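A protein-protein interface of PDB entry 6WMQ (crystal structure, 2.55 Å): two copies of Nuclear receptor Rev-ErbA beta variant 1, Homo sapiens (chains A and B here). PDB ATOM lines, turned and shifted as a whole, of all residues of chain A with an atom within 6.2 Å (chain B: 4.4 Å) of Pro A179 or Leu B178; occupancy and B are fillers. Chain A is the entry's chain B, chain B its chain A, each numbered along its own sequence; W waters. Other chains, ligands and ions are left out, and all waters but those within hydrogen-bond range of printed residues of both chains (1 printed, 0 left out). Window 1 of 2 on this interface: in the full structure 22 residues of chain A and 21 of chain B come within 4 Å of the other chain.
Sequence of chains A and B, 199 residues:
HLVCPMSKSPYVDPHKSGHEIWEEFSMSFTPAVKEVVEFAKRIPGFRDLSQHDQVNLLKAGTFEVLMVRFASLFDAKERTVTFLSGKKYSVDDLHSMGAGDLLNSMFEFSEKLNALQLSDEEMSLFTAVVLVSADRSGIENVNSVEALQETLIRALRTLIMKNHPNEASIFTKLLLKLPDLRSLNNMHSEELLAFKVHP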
ATOM      1  N   LEU A 175      16.132  -5.347  26.032  1.00  0.00           N
ATOM      2  CA  LEU A 175      17.476  -5.674  25.573  1.00  0.00           C
ATOM      3  C   LEU A 175      17.513  -7.040  24.887  1.00  0.00           C
ATOM      4  O   LEU A 175      18.138  -7.197  23.833  1.00  0.00           O
ATOM      5  CB  LEU A 175      18.453  -5.623  26.746  1.00  0.00           C
ATOM      6  CG  LEU A 175      18.927  -4.227  27.182  1.00  0.00           C
ATOM      7  CD1 LEU A 175      20.140  -4.321  28.104  1.00  0.00           C
ATOM      8  CD2 LEU A 175      19.247  -3.361  25.970  1.00  0.00           C
ATOM      9  N   LEU A 176      16.829  -8.036  25.459  1.00  0.00           N
ATOM     10  CA  LEU A 176      16.822  -9.388  24.906  1.00  0.00           C
ATOM     11  C   LEU A 176      16.048  -9.492  23.613  1.00  0.00           C
ATOM     12  O   LEU A 176      16.089 -10.542  22.972  1.00  0.00           O
ATOM     13  CB  LEU A 176      16.244 -10.375  25.915  1.00  0.00           C
ATOM     14  CG  LEU A 176      17.187 -10.527  27.110  1.00  0.00           C
ATOM     15  CD1 LEU A 176      16.705 -11.606  28.079  1.00  0.00           C
ATOM     16  CD2 LEU A 176      18.595 -10.818  26.614  1.00  0.00           C
ATOM     17  N   LYS A 177      15.350  -8.433  23.219  1.00  0.00           N
ATOM     18  CA  LYS A 177      14.730  -8.394  21.910  1.00  0.00           C
ATOM     19  C   LYS A 177      15.729  -8.172  20.784  1.00  0.00           C
ATOM     20  O   LYS A 177      15.380  -8.441  19.627  1.00  0.00           O
ATOM     21  CB  LYS A 177      13.650  -7.319  21.899  1.00  0.00           C
ATOM     22  CG  LYS A 177      12.324  -7.918  22.364  1.00  0.00           C
ATOM     23  CD  LYS A 177      11.300  -6.900  22.774  1.00  0.00           C
ATOM     24  CE  LYS A 177      10.049  -7.617  23.273  1.00  0.00           C
ATOM     25  NZ  LYS A 177      10.394  -8.650  24.299  1.00  0.00           N
ATOM     26  N   LEU A 178      16.971  -7.735  21.097  1.00  0.00           N
ATOM     27  CA  LEU A 178      17.951  -7.392  20.074  1.00  0.00           C
ATOM     28  C   LEU A 178      18.486  -8.656  19.401  1.00  0.00           C
ATOM     29  O   LEU A 178      18.701  -8.647  18.186  1.00  0.00           O
ATOM     30  CB  LEU A 178      19.097  -6.547  20.655  1.00  0.00           C
ATOM     31  CG  LEU A 178      18.700  -5.179  21.233  1.00  0.00           C
ATOM     32  CD1 LEU A 178      19.901  -4.365  21.722  1.00  0.00           C
ATOM     33  CD2 LEU A 178      17.897  -4.382  20.225  1.00  0.00           C
ATOM     34  N   PRO A 179      18.732  -9.756  20.121  1.00  0.00           N
ATOM     35  CA  PRO A 179      19.047 -10.998  19.398  1.00  0.00           C
ATOM     36  C   PRO A 179      17.844 -11.581  18.668  1.00  0.00           C
ATOM     37  O   PRO A 179      18.020 -12.171  17.594  1.00  0.00           O
ATOM     38  CB  PRO A 179      19.587 -11.936  20.492  1.00  0.00           C
ATOM     39  CG  PRO A 179      19.176 -11.352  21.761  1.00  0.00           C
ATOM     40  CD  PRO A 179      19.036  -9.874  21.560  1.00  0.00           C
ATOM     41  N   ASP A 180      16.628 -11.386  19.190  1.00  0.00           N
ATOM     42  CA  ASP A 180      15.428 -11.807  18.467  1.00  0.00           C
ATOM     43  C   ASP A 180      15.305 -11.063  17.142  1.00  0.00           C
ATOM     44  O   ASP A 180      15.102 -11.679  16.089  1.00  0.00           O
ATOM     45  CB  ASP A 180      14.181 -11.588  19.332  1.00  0.00           C
ATOM     46  CG  ASP A 180      14.176 -12.458  20.598  1.00  0.00           C
ATOM     47  OD1 ASP A 180      13.146 -12.477  21.314  1.00  0.00           O
ATOM     48  OD2 ASP A 180      15.198 -13.134  20.881  1.00  0.00           O
ATOM     49  N   LEU A 181      15.433  -9.731  17.177  1.00  0.00           N
ATOM     50  CA  LEU A 181      15.343  -8.948  15.949  1.00  0.00           C
ATOM     51  C   LEU A 181      16.424  -9.360  14.972  1.00  0.00           C
ATOM     52  O   LEU A 181      16.201  -9.378  13.754  1.00  0.00           O
ATOM     53  CB  LEU A 181      15.465  -7.462  16.249  1.00  0.00           C
ATOM     54  CG  LEU A 181      14.223  -6.880  16.896  1.00  0.00           C
ATOM     55  CD1 LEU A 181      14.676  -5.812  17.892  1.00  0.00           C
ATOM     56  CD2 LEU A 181      13.258  -6.325  15.866  1.00  0.00           C
ATOM     57  N   ARG A 182      17.603  -9.704  15.492  1.00  0.00           N
ATOM     58  CA  ARG A 182      18.681 -10.119  14.613  1.00  0.00           C
ATOM     59  C   ARG A 182      18.343 -11.449  13.952  1.00  0.00           C
ATOM     60  O   ARG A 182      18.616 -11.643  12.771  1.00  0.00           O
ATOM     61  CB  ARG A 182      20.000 -10.166  15.394  1.00  0.00           C
ATOM     62  CG  ARG A 182      21.242 -10.446  14.564  1.00  0.00           C
ATOM     63  CD  ARG A 182      21.507  -9.386  13.477  1.00  0.00           C
ATOM     64  NE  ARG A 182      21.228  -8.037  13.949  1.00  0.00           N
ATOM     65  CZ  ARG A 182      22.053  -7.316  14.707  1.00  0.00           C
ATOM     66  NH1 ARG A 182      23.237  -7.806  15.086  1.00  0.00           N
ATOM     67  NH2 ARG A 182      21.690  -6.094  15.090  1.00  0.00           N
ATOM     68  N   SER A 183      17.681 -12.350  14.672  1.00  0.00           N
ATOM     69  CA  SER A 183      17.331 -13.639  14.090  1.00  0.00           C
ATOM     70  C   SER A 183      16.226 -13.511  13.050  1.00  0.00           C
ATOM     71  O   SER A 183      16.264 -14.186  12.018  1.00  0.00           O
ATOM     72  CB  SER A 183      16.919 -14.610  15.186  1.00  0.00           C
ATOM     73  OG  SER A 183      18.067 -15.190  15.746  1.00  0.00           O
ATOM     74  N   LEU A 184      15.216 -12.681  13.315  1.00  0.00           N
ATOM     75  CA  LEU A 184      14.198 -12.406  12.306  1.00  0.00           C
ATOM     76  C   LEU A 184      14.837 -11.813  11.052  1.00  0.00           C
ATOM     77  O   LEU A 184      14.538 -12.245   9.926  1.00  0.00           O
ATOM     78  CB  LEU A 184      13.126 -11.465  12.871  1.00  0.00           C
ATOM     79  CG  LEU A 184      12.342 -11.890  14.130  1.00  0.00           C
ATOM     80  CD1 LEU A 184      11.433 -10.763  14.590  1.00  0.00           C
ATOM     81  CD2 LEU A 184      11.520 -13.175  13.985  1.00  0.00           C
ATOM     82  N   ASN A 186      17.846 -12.335   9.958  1.00  0.00           N
ATOM     83  CA  ASN A 186      18.503 -13.393   9.198  1.00  0.00           C
ATOM     84  C   ASN A 186      17.488 -14.329   8.554  1.00  0.00           C
ATOM     85  O   ASN A 186      17.662 -14.732   7.397  1.00  0.00           O
ATOM     86  CB  ASN A 186      19.476 -14.159  10.087  1.00  0.00           C
ATOM     87  CG  ASN A 186      20.352 -13.233  10.917  1.00  0.00           C
ATOM     88  OD1 ASN A 186      20.494 -13.421  12.120  1.00  0.00           O
ATOM     89  ND2 ASN A 186      20.959 -12.247  10.280  1.00  0.00           N
ATOM     90  N   VAL B 130      24.010 -17.094  27.166  1.00  0.00           N
ATOM     91  CA  VAL B 130      24.146 -17.198  25.721  1.00  0.00           C
ATOM     92  C   VAL B 130      23.431 -18.439  25.217  1.00  0.00           C
ATOM     93  O   VAL B 130      22.769 -18.409  24.174  1.00  0.00           O
ATOM     94  CB  VAL B 130      25.634 -17.204  25.323  1.00  0.00           C
ATOM     95  CG1 VAL B 130      25.808 -17.671  23.874  1.00  0.00           C
ATOM     96  CG2 VAL B 130      26.287 -15.837  25.578  1.00  0.00           C
ATOM     97  N   SER B 133      19.659 -18.090  25.306  1.00  0.00           N
ATOM     98  CA  SER B 133      19.256 -17.014  24.413  1.00  0.00           C
ATOM     99  C   SER B 133      19.297 -17.429  22.957  1.00  0.00           C
ATOM    100  O   SER B 133      19.137 -16.568  22.073  1.00  0.00           O
ATOM    101  CB  SER B 133      20.146 -15.789  24.608  1.00  0.00           C
ATOM    102  OG  SER B 133      19.793 -15.095  25.783  1.00  0.00           O
ATOM    103  N   LEU B 174      27.593  -6.906  28.447  1.00  0.00           N
ATOM    104  CA  LEU B 174      27.485  -8.338  28.184  1.00  0.00           C
ATOM    105  C   LEU B 174      26.192  -8.683  27.448  1.00  0.00           C
ATOM    106  O   LEU B 174      26.182  -9.581  26.600  1.00  0.00           O
ATOM    107  CB  LEU B 174      27.580  -9.119  29.489  1.00  0.00           C
ATOM    108  CG  LEU B 174      28.975  -9.216  30.097  1.00  0.00           C
ATOM    109  CD1 LEU B 174      28.905  -9.855  31.480  1.00  0.00           C
ATOM    110  CD2 LEU B 174      29.907 -10.003  29.174  1.00  0.00           C
ATOM    111  N   LEU B 175      25.090  -7.991  27.752  1.00  0.00           N
ATOM    112  CA  LEU B 175      23.851  -8.283  27.034  1.00  0.00           C
ATOM    113  C   LEU B 175      23.960  -7.859  25.578  1.00  0.00           C
ATOM    114  O   LEU B 175      23.519  -8.578  24.676  1.00  0.00           O
ATOM    115  CB  LEU B 175      22.665  -7.588  27.690  1.00  0.00           C
ATOM    116  CG  LEU B 175      22.213  -8.127  29.049  1.00  0.00           C
ATOM    117  CD1 LEU B 175      20.823  -7.584  29.404  1.00  0.00           C
ATOM    118  CD2 LEU B 175      22.224  -9.643  29.075  1.00  0.00           C
ATOM    119  N   LEU B 176      24.572  -6.704  25.333  1.00  0.00           N
ATOM    120  CA  LEU B 176      24.682  -6.175  23.990  1.00  0.00           C
ATOM    121  C   LEU B 176      25.614  -7.002  23.121  1.00  0.00           C
ATOM    122  O   LEU B 176      25.661  -6.794  21.913  1.00  0.00           O
ATOM    123  CB  LEU B 176      25.134  -4.721  24.065  1.00  0.00           C
ATOM    124  CG  LEU B 176      24.111  -3.817  24.753  1.00  0.00           C
ATOM    125  CD1 LEU B 176      24.691  -2.424  24.930  1.00  0.00           C
ATOM    126  CD2 LEU B 176      22.802  -3.768  23.972  1.00  0.00           C
ATOM    127  N   LYS B 177      26.330  -7.956  23.702  1.00  0.00           N
ATOM    128  CA  LYS B 177      27.033  -8.925  22.890  1.00  0.00           C
ATOM    129  C   LYS B 177      26.095  -9.955  22.270  1.00  0.00           C
ATOM    130  O   LYS B 177      26.455 -10.549  21.249  1.00  0.00           O
ATOM    131  CB  LYS B 177      28.106  -9.607  23.733  1.00  0.00           C
ATOM    132  CG  LYS B 177      29.324  -8.716  23.908  1.00  0.00           C
ATOM    133  CD  LYS B 177      30.279  -9.237  24.956  1.00  0.00           C
ATOM    134  CE  LYS B 177      31.691  -8.753  24.678  1.00  0.00           C
ATOM    135  NZ  LYS B 177      31.865  -7.264  24.753  1.00  0.00           N
ATOM    136  N   LEU B 178      24.902 -10.175  22.849  1.00  0.00           N
ATOM    137  CA  LEU B 178      24.008 -11.194  22.296  1.00  0.00           C
ATOM    138  C   LEU B 178      23.695 -10.965  20.824  1.00  0.00           C
ATOM    139  O   LEU B 178      23.854 -11.913  20.041  1.00  0.00           O
ATOM    140  CB  LEU B 178      22.728 -11.307  23.133  1.00  0.00           C
ATOM    141  CG  LEU B 178      22.973 -11.781  24.560  1.00  0.00           C
ATOM    142  CD1 LEU B 178      21.661 -12.123  25.279  1.00  0.00           C
ATOM    143  CD2 LEU B 178      23.923 -12.962  24.558  1.00  0.00           C
ATOM    144  N   PRO B 179      23.290  -9.774  20.362  1.00  0.00           N
ATOM    145  CA  PRO B 179      23.073  -9.626  18.908  1.00  0.00           C
ATOM    146  C   PRO B 179      24.346  -9.781  18.093  1.00  0.00           C
ATOM    147  O   PRO B 179      24.276 -10.287  16.963  1.00  0.00           O
ATOM    148  CB  PRO B 179      22.469  -8.221  18.765  1.00  0.00           C
ATOM    149  CG  PRO B 179      22.789  -7.526  20.007  1.00  0.00           C
ATOM    150  CD  PRO B 179      22.923  -8.545  21.094  1.00  0.00           C
ATOM    151  N   ASP B 180      25.499  -9.380  18.653  1.00  0.00           N
ATOM    152  CA  ASP B 180      26.790  -9.537  17.980  1.00  0.00           C
ATOM    153  C   ASP B 180      27.121 -11.011  17.750  1.00  0.00           C
ATOM    154  O   ASP B 180      27.585 -11.393  16.669  1.00  0.00           O
ATOM    155  CB  ASP B 180      27.896  -8.862  18.805  1.00  0.00           C
ATOM    156  CG  ASP B 180      27.786  -7.323  18.819  1.00  0.00           C
ATOM    157  OD1 ASP B 180      26.944  -6.766  18.071  1.00  0.00           O
ATOM    158  OD2 ASP B 180      28.532  -6.663  19.591  1.00  0.00           O
ATOM    159  N   LEU B 181      26.898 -11.853  18.768  1.00  0.00           N
ATOM    160  CA  LEU B 181      27.060 -13.301  18.616  1.00  0.00           C
ATOM    161  C   LEU B 181      26.051 -13.895  17.626  1.00  0.00           C
ATOM    162  O   LEU B 181      26.320 -14.919  16.984  1.00  0.00           O
ATOM    163  CB  LEU B 181      26.908 -13.980  19.978  1.00  0.00           C
ATOM    164  CG  LEU B 181      28.140 -14.079  20.875  1.00  0.00           C
ATOM    165  CD1 LEU B 181      27.756 -13.977  22.357  1.00  0.00           C
ATOM    166  CD2 LEU B 181      28.795 -15.408  20.613  1.00  0.00           C
ATOM    167  N   ARG B 182      24.886 -13.276  17.495  1.00  0.00           N
ATOM    168  CA  ARG B 182      23.899 -13.816  16.582  1.00  0.00           C
ATOM    169  C   ARG B 182      24.282 -13.482  15.144  1.00  0.00           C
ATOM    170  O   ARG B 182      24.094 -14.313  14.257  1.00  0.00           O
ATOM    171  CB  ARG B 182      22.498 -13.311  16.978  1.00  0.00           C
ATOM    172  CG  ARG B 182      21.342 -13.836  16.141  1.00  0.00           C
ATOM    173  CD  ARG B 182      21.012 -15.345  16.347  1.00  0.00           C
ATOM    174  NE  ARG B 182      21.138 -15.856  17.712  1.00  0.00           N
ATOM    175  CZ  ARG B 182      20.296 -15.593  18.714  1.00  0.00           C
ATOM    176  NH1 ARG B 182      19.242 -14.799  18.534  1.00  0.00           N
ATOM    177  NH2 ARG B 182      20.509 -16.132  19.913  1.00  0.00           N
HETATM  178  O   HOH W   1      16.665 -15.079  20.314  1.00  0.00           O
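NH1 of Arg B182 lies close to OG of Ser A183, at 3.1 Å.
The guanidinium group of Arg B182 sits at hydrogen-bond distance from the backbone carbonyl oxygen of Pro A179.
O of Pro B179 sits at hydrogen-bond distance from NH1 of Arg A182 (3.3 Å).
NH2 of Arg B182 is in hydrogen-bond range of O of Ser B133 (2.6 Å).
O of Arg A182 lies close to OD1 of Asn A186 (2.7 Å).
Among the printed residues, pairs that only touch across the chains: Leu A175 with Leu B175, Leu A176 with Leu B178, Leu A178 with Leu B176, Leu A178 with Pro B179, Pro A179 with Leu B178 and Arg A182 with Arg B182.
Printed residues of chain B within 4 Å of Pro A179: Leu B178 (3.8 Å) and Arg B182 (3.0 Å).
Of chain A, only Leu A176 and Pro A179 come within 4 Å of Leu B178.
Printed residues of chain B within 4 Å of Ser A183: Arg B182.
Printed residues of chain A within 4 Å of Leu B175: Leu A175.
Printed residues of chain B within 4 Å of Leu A175: Leu B175 (3.6 Å).
Printed residues of chain B within 4 Å of Leu A176: Leu B178.
Leu A181 touches none of the printed residues of chain B.
Lys A177 touches none of the printed residues of chain B.
The nearest residue of chain B that does not touch Pro A179 is Pro B179 (4.1 Å).
Printed residues of chain A that touch a printed residue of chain B: Leu A175, Leu A176, Leu A178, Pro A179, Arg A182 and Ser A183.
Along chain A the printed residues that touch a printed residue of chain B span positions 175 to 183.
Among the printed residues, 9 pairs touch across the chains.
Among the printed residues, no Asp or Glu carboxylate lies within 4 Å of a Lys or Arg side-chain nitrogen of the other chain.
Leu A176 touches Leu B178, and with the chains exchanged Leu A178 touches Leu B176.
Leu A178 touches Pro B179, and with the chains exchanged Pro A179 touches Leu B178.
Pro A179 touches Arg B182, and with the chains exchanged Arg A182 touches Pro B179.
Arg A182 touches its own counterpart, Arg B182.
8 positions are printed for both chains.
Of the 9 pairs that touch across the chains among the printed residues, 8 have their exchanged pair printed and touching as well.
Water W1 lies within hydrogen-bond range of the side-chain carboxylate of Asp A180 (2.5 Å), the guanidinium group of Arg B182 (3.1 Å) and the backbone carbonyl oxygen of Ser B133 (3.4 Å).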
